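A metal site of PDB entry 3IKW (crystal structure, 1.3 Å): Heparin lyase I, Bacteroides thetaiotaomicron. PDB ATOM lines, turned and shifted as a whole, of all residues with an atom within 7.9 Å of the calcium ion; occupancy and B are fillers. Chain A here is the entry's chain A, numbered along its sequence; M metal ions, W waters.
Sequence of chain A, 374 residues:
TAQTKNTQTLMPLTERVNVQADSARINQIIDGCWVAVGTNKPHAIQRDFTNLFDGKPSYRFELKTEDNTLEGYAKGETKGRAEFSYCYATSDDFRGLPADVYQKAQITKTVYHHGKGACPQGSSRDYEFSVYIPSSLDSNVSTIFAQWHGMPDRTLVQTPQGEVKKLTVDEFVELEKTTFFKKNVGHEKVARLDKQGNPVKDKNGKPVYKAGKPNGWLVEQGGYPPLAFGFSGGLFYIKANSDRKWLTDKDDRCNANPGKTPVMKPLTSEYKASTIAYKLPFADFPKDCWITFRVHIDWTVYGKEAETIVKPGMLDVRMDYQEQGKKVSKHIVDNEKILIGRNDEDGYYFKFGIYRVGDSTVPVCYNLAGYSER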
ATOM      1  N   GLN A 121      12.300  12.466   3.337  1.00  0.00           N
ATOM      2  CA  GLN A 121      13.292  12.458   2.254  1.00  0.00           C
ATOM      3  C   GLN A 121      14.626  12.962   2.725  1.00  0.00           C
ATOM      4  O   GLN A 121      14.675  13.947   3.444  1.00  0.00           O
ATOM      5  CB  GLN A 121      12.839  13.402   1.145  1.00  0.00           C
ATOM      6  CG  GLN A 121      11.794  12.772   0.269  1.00  0.00           C
ATOM      7  CD  GLN A 121      12.391  11.707  -0.602  1.00  0.00           C
ATOM      8  OE1 GLN A 121      13.518  11.869  -1.102  1.00  0.00           O
ATOM      9  NE2 GLN A 121      11.654  10.626  -0.828  1.00  0.00           N
ATOM     10  N   MET A 151       6.506   6.374  -0.082  1.00  0.00           N
ATOM     11  CA  MET A 151       5.143   6.835   0.157  1.00  0.00           C
ATOM     12  C   MET A 151       4.716   7.815  -0.926  1.00  0.00           C
ATOM     13  O   MET A 151       4.394   8.963  -0.654  1.00  0.00           O
ATOM     14  CB  MET A 151       5.030   7.475   1.540  1.00  0.00           C
ATOM     15  CG  MET A 151       5.360   6.490   2.646  1.00  0.00           C
ATOM     16  SD  MET A 151       5.398   7.226   4.303  1.00  0.00           S
ATOM     17  CE  MET A 151       3.655   7.617   4.549  1.00  0.00           C
ATOM     18  N   PRO A 152       4.689   7.366  -2.186  1.00  0.00           N
ATOM     19  CA  PRO A 152       4.269   8.313  -3.225  1.00  0.00           C
ATOM     20  C   PRO A 152       2.841   8.803  -3.025  1.00  0.00           C
ATOM     21  O   PRO A 152       1.998   8.102  -2.478  1.00  0.00           O
ATOM     22  CB  PRO A 152       4.362   7.500  -4.524  1.00  0.00           C
ATOM     23  CG  PRO A 152       4.344   6.056  -4.070  1.00  0.00           C
ATOM     24  CD  PRO A 152       5.011   6.043  -2.724  1.00  0.00           C
ATOM     25  N   ASP A 153       2.600  10.011  -3.495  1.00  0.00           N
ATOM     26  CA  ASP A 153       1.288  10.658  -3.399  1.00  0.00           C
ATOM     27  C   ASP A 153       0.723  10.647  -4.826  1.00  0.00           C
ATOM     28  O   ASP A 153       1.306  11.244  -5.744  1.00  0.00           O
ATOM     29  CB  ASP A 153       1.501  12.075  -2.872  1.00  0.00           C
ATOM     30  CG  ASP A 153       0.240  12.900  -2.808  1.00  0.00           C
ATOM     31  OD1 ASP A 153      -0.700  12.643  -3.570  1.00  0.00           O
ATOM     32  OD2 ASP A 153       0.220  13.861  -2.007  1.00  0.00           O
ATOM     33  N   LEU A 156       0.325  13.340  -7.786  1.00  0.00           N
ATOM     34  CA  LEU A 156       1.297  13.643  -8.836  1.00  0.00           C
ATOM     35  C   LEU A 156       0.939  12.795 -10.023  1.00  0.00           C
ATOM     36  O   LEU A 156       0.940  11.544  -9.936  1.00  0.00           O
ATOM     37  CB  LEU A 156       2.730  13.335  -8.422  1.00  0.00           C
ATOM     38  CG  LEU A 156       3.754  13.799  -9.469  1.00  0.00           C
ATOM     39  CD1 LEU A 156       3.841  15.333  -9.528  1.00  0.00           C
ATOM     40  CD2 LEU A 156       5.162  13.249  -9.175  1.00  0.00           C
ATOM     41  N   GLU A 220       0.987   8.597  -9.708  1.00  0.00           N
ATOM     42  CA  GLU A 220       2.144   7.960  -9.108  1.00  0.00           C
ATOM     43  C   GLU A 220       1.726   6.993  -8.007  1.00  0.00           C
ATOM     44  O   GLU A 220       1.401   7.417  -6.907  1.00  0.00           O
ATOM     45  CB  GLU A 220       3.152   8.977  -8.538  1.00  0.00           C
ATOM     46  CG  GLU A 220       4.501   8.262  -8.333  1.00  0.00           C
ATOM     47  CD  GLU A 220       5.708   9.161  -8.127  1.00  0.00           C
ATOM     48  OE1 GLU A 220       5.606  10.180  -7.430  1.00  0.00           O
ATOM     49  OE2 GLU A 220       6.812   8.795  -8.598  1.00  0.00           O
ATOM     50  N   ASP A 243      15.230   5.319  -7.418  1.00  0.00           N
ATOM     51  CA  ASP A 243      14.513   5.822  -8.588  1.00  0.00           C
ATOM     52  C   ASP A 243      14.597   7.333  -8.560  1.00  0.00           C
ATOM     53  O   ASP A 243      14.007   7.957  -7.671  1.00  0.00           O
ATOM     54  CB  ASP A 243      13.057   5.408  -8.493  1.00  0.00           C
ATOM     55  CG  ASP A 243      12.261   5.714  -9.734  1.00  0.00           C
ATOM     56  OD1 ASP A 243      12.733   6.436 -10.622  1.00  0.00           O
ATOM     57  OD2 ASP A 243      11.123   5.199  -9.806  1.00  0.00           O
ATOM     58  N   ARG A 244      15.329   7.905  -9.502  1.00  0.00           N
ATOM     59  CA  ARG A 244      15.513   9.369  -9.509  1.00  0.00           C
ATOM     60  C   ARG A 244      14.501  10.097 -10.388  1.00  0.00           C
ATOM     61  O   ARG A 244      14.471  11.334 -10.401  1.00  0.00           O
ATOM     62  CB  ARG A 244      16.928   9.757  -9.963  1.00  0.00           C
ATOM     63  CG  ARG A 244      17.162   9.614 -11.444  1.00  0.00           C
ATOM     64  CD  ARG A 244      18.619   9.943 -11.858  1.00  0.00           C
ATOM     65  NE  ARG A 244      18.816   9.625 -13.268  1.00  0.00           N
ATOM     66  CZ  ARG A 244      18.507  10.439 -14.268  1.00  0.00           C
ATOM     67  NH1 ARG A 244      18.016  11.643 -14.013  1.00  0.00           N
ATOM     68  NH2 ARG A 244      18.672  10.055 -15.524  1.00  0.00           N
ATOM     69  N   LYS A 245      13.671   9.351 -11.107  1.00  0.00           N
ATOM     70  CA  LYS A 245      12.645   9.986 -11.932  1.00  0.00           C
ATOM     71  C   LYS A 245      11.682  10.723 -11.012  1.00  0.00           C
ATOM     72  O   LYS A 245      11.415  10.280  -9.894  1.00  0.00           O
ATOM     73  CB  LYS A 245      11.902   8.968 -12.801  1.00  0.00           C
ATOM     74  CG  LYS A 245      11.327   9.568 -14.090  1.00  0.00           C
ATOM     75  CD  LYS A 245      10.943   8.488 -15.084  1.00  0.00           C
ATOM     76  CE  LYS A 245      10.801   9.068 -16.486  1.00  0.00           C
ATOM     77  NZ  LYS A 245       9.648  10.000 -16.546  1.00  0.00           N
ATOM     78  N   TRP A 246      11.180  11.881 -11.442  1.00  0.00           N
ATOM     79  CA  TRP A 246      10.208  12.593 -10.604  1.00  0.00           C
ATOM     80  C   TRP A 246       8.865  11.853 -10.579  1.00  0.00           C
ATOM     81  O   TRP A 246       8.346  11.582  -9.500  1.00  0.00           O
ATOM     82  CB  TRP A 246      10.073  14.049 -11.075  1.00  0.00           C
ATOM     83  CG  TRP A 246       9.115  14.898 -10.277  1.00  0.00           C
ATOM     84  CD1 TRP A 246       8.078  15.621 -10.793  1.00  0.00           C
ATOM     85  CD2 TRP A 246       9.117  15.151  -8.862  1.00  0.00           C
ATOM     86  NE1 TRP A 246       7.433  16.283  -9.785  1.00  0.00           N
ATOM     87  CE2 TRP A 246       8.042  16.024  -8.587  1.00  0.00           C
ATOM     88  CE3 TRP A 246       9.906  14.709  -7.795  1.00  0.00           C
ATOM     89  CZ2 TRP A 246       7.747  16.465  -7.326  1.00  0.00           C
ATOM     90  CZ3 TRP A 246       9.611  15.157  -6.521  1.00  0.00           C
ATOM     91  CH2 TRP A 246       8.541  16.036  -6.300  1.00  0.00           C
ATOM     92  N   LEU A 247       8.312  11.529 -11.742  1.00  0.00           N
ATOM     93  CA  LEU A 247       7.179  10.604 -11.805  1.00  0.00           C
ATOM     94  C   LEU A 247       7.720   9.246 -12.234  1.00  0.00           C
ATOM     95  O   LEU A 247       8.219   9.086 -13.347  1.00  0.00           O
ATOM     96  CB  LEU A 247       6.130  11.101 -12.819  1.00  0.00           C
ATOM     97  CG  LEU A 247       4.970  10.157 -13.067  1.00  0.00           C
ATOM     98  CD1 LEU A 247       4.170   9.885 -11.788  1.00  0.00           C
ATOM     99  CD2 LEU A 247       4.047  10.689 -14.196  1.00  0.00           C
ATOM    100  N   THR A 248       7.646   8.268 -11.328  1.00  0.00           N
ATOM    101  CA  THR A 248       8.188   6.944 -11.613  1.00  0.00           C
ATOM    102  C   THR A 248       7.570   6.360 -12.861  1.00  0.00           C
ATOM    103  O   THR A 248       6.377   6.490 -13.092  1.00  0.00           O
ATOM    104  CB  THR A 248       7.935   6.034 -10.421  1.00  0.00           C
ATOM    105  OG1 THR A 248       8.823   6.414  -9.369  1.00  0.00           O
ATOM    106  CG2 THR A 248       8.165   4.559 -10.753  1.00  0.00           C
ATOM    107  N   ASP A 249       8.397   5.739 -13.688  1.00  0.00           N
ATOM    108  CA  ASP A 249       7.934   5.007 -14.864  1.00  0.00           C
ATOM    109  C   ASP A 249       7.755   3.543 -14.482  1.00  0.00           C
ATOM    110  O   ASP A 249       8.736   2.820 -14.250  1.00  0.00           O
ATOM    111  CB  ASP A 249       8.986   5.166 -15.981  1.00  0.00           C
ATOM    112  CG  ASP A 249       8.642   4.374 -17.225  1.00  0.00           C
ATOM    113  OD1 ASP A 249       7.577   3.724 -17.262  1.00  0.00           O
ATOM    114  OD2 ASP A 249       9.449   4.402 -18.182  1.00  0.00           O
ATOM    115  N   LYS A 304      14.222  16.477  -6.871  1.00  0.00           N
ATOM    116  CA  LYS A 304      12.812  16.694  -7.225  1.00  0.00           C
ATOM    117  C   LYS A 304      12.620  16.794  -8.731  1.00  0.00           C
ATOM    118  O   LYS A 304      13.054  15.913  -9.457  1.00  0.00           O
ATOM    119  CB  LYS A 304      12.202  17.885  -6.484  1.00  0.00           C
ATOM    120  CG  LYS A 304      12.348  17.756  -4.984  1.00  0.00           C
ATOM    121  CD  LYS A 304      11.512  18.796  -4.252  1.00  0.00           C
ATOM    122  CE  LYS A 304      11.985  18.957  -2.827  1.00  0.00           C
ATOM    123  NZ  LYS A 304      11.645  17.775  -1.981  1.00  0.00           N
ATOM    124  N   ARG A 342      13.643   6.999  -3.280  1.00  0.00           N
ATOM    125  CA  ARG A 342      12.744   7.351  -4.380  1.00  0.00           C
ATOM    126  C   ARG A 342      12.624   8.856  -4.438  1.00  0.00           C
ATOM    127  O   ARG A 342      12.504   9.511  -3.382  1.00  0.00           O
ATOM    128  CB  ARG A 342      11.316   6.866  -4.090  1.00  0.00           C
ATOM    129  CG  ARG A 342      11.039   5.412  -4.224  1.00  0.00           C
ATOM    130  CD  ARG A 342       9.545   5.126  -3.924  1.00  0.00           C
ATOM    131  NE  ARG A 342       8.671   6.045  -4.650  1.00  0.00           N
ATOM    132  CZ  ARG A 342       8.293   5.859  -5.901  1.00  0.00           C
ATOM    133  NH1 ARG A 342       8.690   4.766  -6.559  1.00  0.00           N
ATOM    134  NH2 ARG A 342       7.533   6.746  -6.515  1.00  0.00           N
ATOM    135  N   ASN A 343      12.596   9.403  -5.646  1.00  0.00           N
ATOM    136  CA  ASN A 343      12.421  10.838  -5.817  1.00  0.00           C
ATOM    137  C   ASN A 343      10.960  11.235  -5.676  1.00  0.00           C
ATOM    138  O   ASN A 343      10.260  11.365  -6.672  1.00  0.00           O
ATOM    139  CB  ASN A 343      12.966  11.269  -7.177  1.00  0.00           C
ATOM    140  CG  ASN A 343      13.011  12.780  -7.336  1.00  0.00           C
ATOM    141  OD1 ASN A 343      12.798  13.534  -6.390  1.00  0.00           O
ATOM    142  ND2 ASN A 343      13.291  13.213  -8.563  1.00  0.00           N
ATOM    143  N   ASP A 344      10.505  11.372  -4.420  1.00  0.00           N
ATOM    144  CA  ASP A 344       9.140  11.764  -4.068  1.00  0.00           C
ATOM    145  C   ASP A 344       9.214  12.953  -3.109  1.00  0.00           C
ATOM    146  O   ASP A 344      10.263  13.243  -2.518  1.00  0.00           O
ATOM    147  CB  ASP A 344       8.407  10.638  -3.303  1.00  0.00           C
ATOM    148  CG  ASP A 344       8.061   9.432  -4.160  1.00  0.00           C
ATOM    149  OD1 ASP A 344       8.071   9.477  -5.413  1.00  0.00           O
ATOM    150  OD2 ASP A 344       7.757   8.406  -3.545  1.00  0.00           O
ATOM    151  N   GLU A 345       8.090  13.619  -2.917  1.00  0.00           N
ATOM    152  CA  GLU A 345       8.012  14.610  -1.861  1.00  0.00           C
ATOM    153  C   GLU A 345       8.056  13.966  -0.475  1.00  0.00           C
ATOM    154  O   GLU A 345       8.700  14.479   0.444  1.00  0.00           O
ATOM    155  CB  GLU A 345       6.711  15.399  -2.028  1.00  0.00           C
ATOM    156  CG  GLU A 345       6.521  16.501  -1.007  1.00  0.00           C
ATOM    157  CD  GLU A 345       7.491  17.646  -1.179  1.00  0.00           C
ATOM    158  OE1 GLU A 345       7.997  17.834  -2.315  1.00  0.00           O
ATOM    159  OE2 GLU A 345       7.750  18.365  -0.184  1.00  0.00           O
ATOM    160  N   ASP A 346       7.383  12.821  -0.323  1.00  0.00           N
ATOM    161  CA  ASP A 346       7.222  12.156   0.953  1.00  0.00           C
ATOM    162  C   ASP A 346       8.277  11.082   1.156  1.00  0.00           C
ATOM    163  O   ASP A 346       9.024  10.757   0.242  1.00  0.00           O
ATOM    164  CB  ASP A 346       5.806  11.602   1.053  1.00  0.00           C
ATOM    165  CG  ASP A 346       4.755  12.682   0.879  1.00  0.00           C
ATOM    166  OD1 ASP A 346       4.727  13.585   1.731  1.00  0.00           O
ATOM    167  OD2 ASP A 346       4.005  12.627  -0.097  1.00  0.00           O
HETATM  168 CA    CA M   1       8.128  10.493  -7.486  1.00  0.00          CA
HETATM  169  O   HOH W   1       7.479  12.685  -6.808  1.00  0.00           O
HETATM  170  O   HOH W   2       9.714   8.808  -8.242  1.00  0.00           O
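NE2 of Gln 121 lies close to O of Asp 344 (3.4 Å). OG1 of Thr 248 lies within hydrogen-bond range of NH2 of Arg 342 (3.1 Å). The side-chain amide nitrogen (NE2) of Gln 121 is in hydrogen-bond range of the backbone carbonyl oxygen (O) of Arg 342, at 2.9 Å. The side-chain amide nitrogen (ND2) of Asn 343 sits at hydrogen-bond distance from the backbone carbonyl oxygen (O) of Lys 304 (2.9 Å). The side-chain carboxylate (OD2) of Asp 344 lies within salt-bridge range of the guanidinium group (NE) of Arg 342, 2.8 Å away. N of Thr 248 sits close to OE2 of Glu 220 (2.9 Å). N of Asn 343 sits at hydrogen-bond distance from O of Asp 243. OE2 of Glu 220 lies close to NH2 of Arg 342, 3.0 Å away.
O of Trp 246 is bound to the calcium ion, 2.3 Å away. OD1 of Asp 344 binds the calcium ion. Water W1 binds the calcium ion (2.4 Å). The calcium ion is bound by OE2 of Glu 220. Water W2 binds the calcium ion. The calcium ion is bound by the backbone carbonyl oxygen (O) of Asn 343, 2.4 Å away. The calcium ion is bound by the side-chain carboxylate (OE1) of Glu 220 (2.5 Å).
Water W2 lies within hydrogen-bond range of the backbone carbonyl oxygen (O) of Lys 245 (2.8 Å), the side-chain hydroxyl (OG1) of Thr 248 (2.8 Å) and the guanidinium group (NH2) of Arg 342 (3.5 Å).
Residues that only touch the calcium ion: Arg 342 (3.9 Å). The nearest printed residue that does not touch the calcium ion is Lys 245 (4.1 Å).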
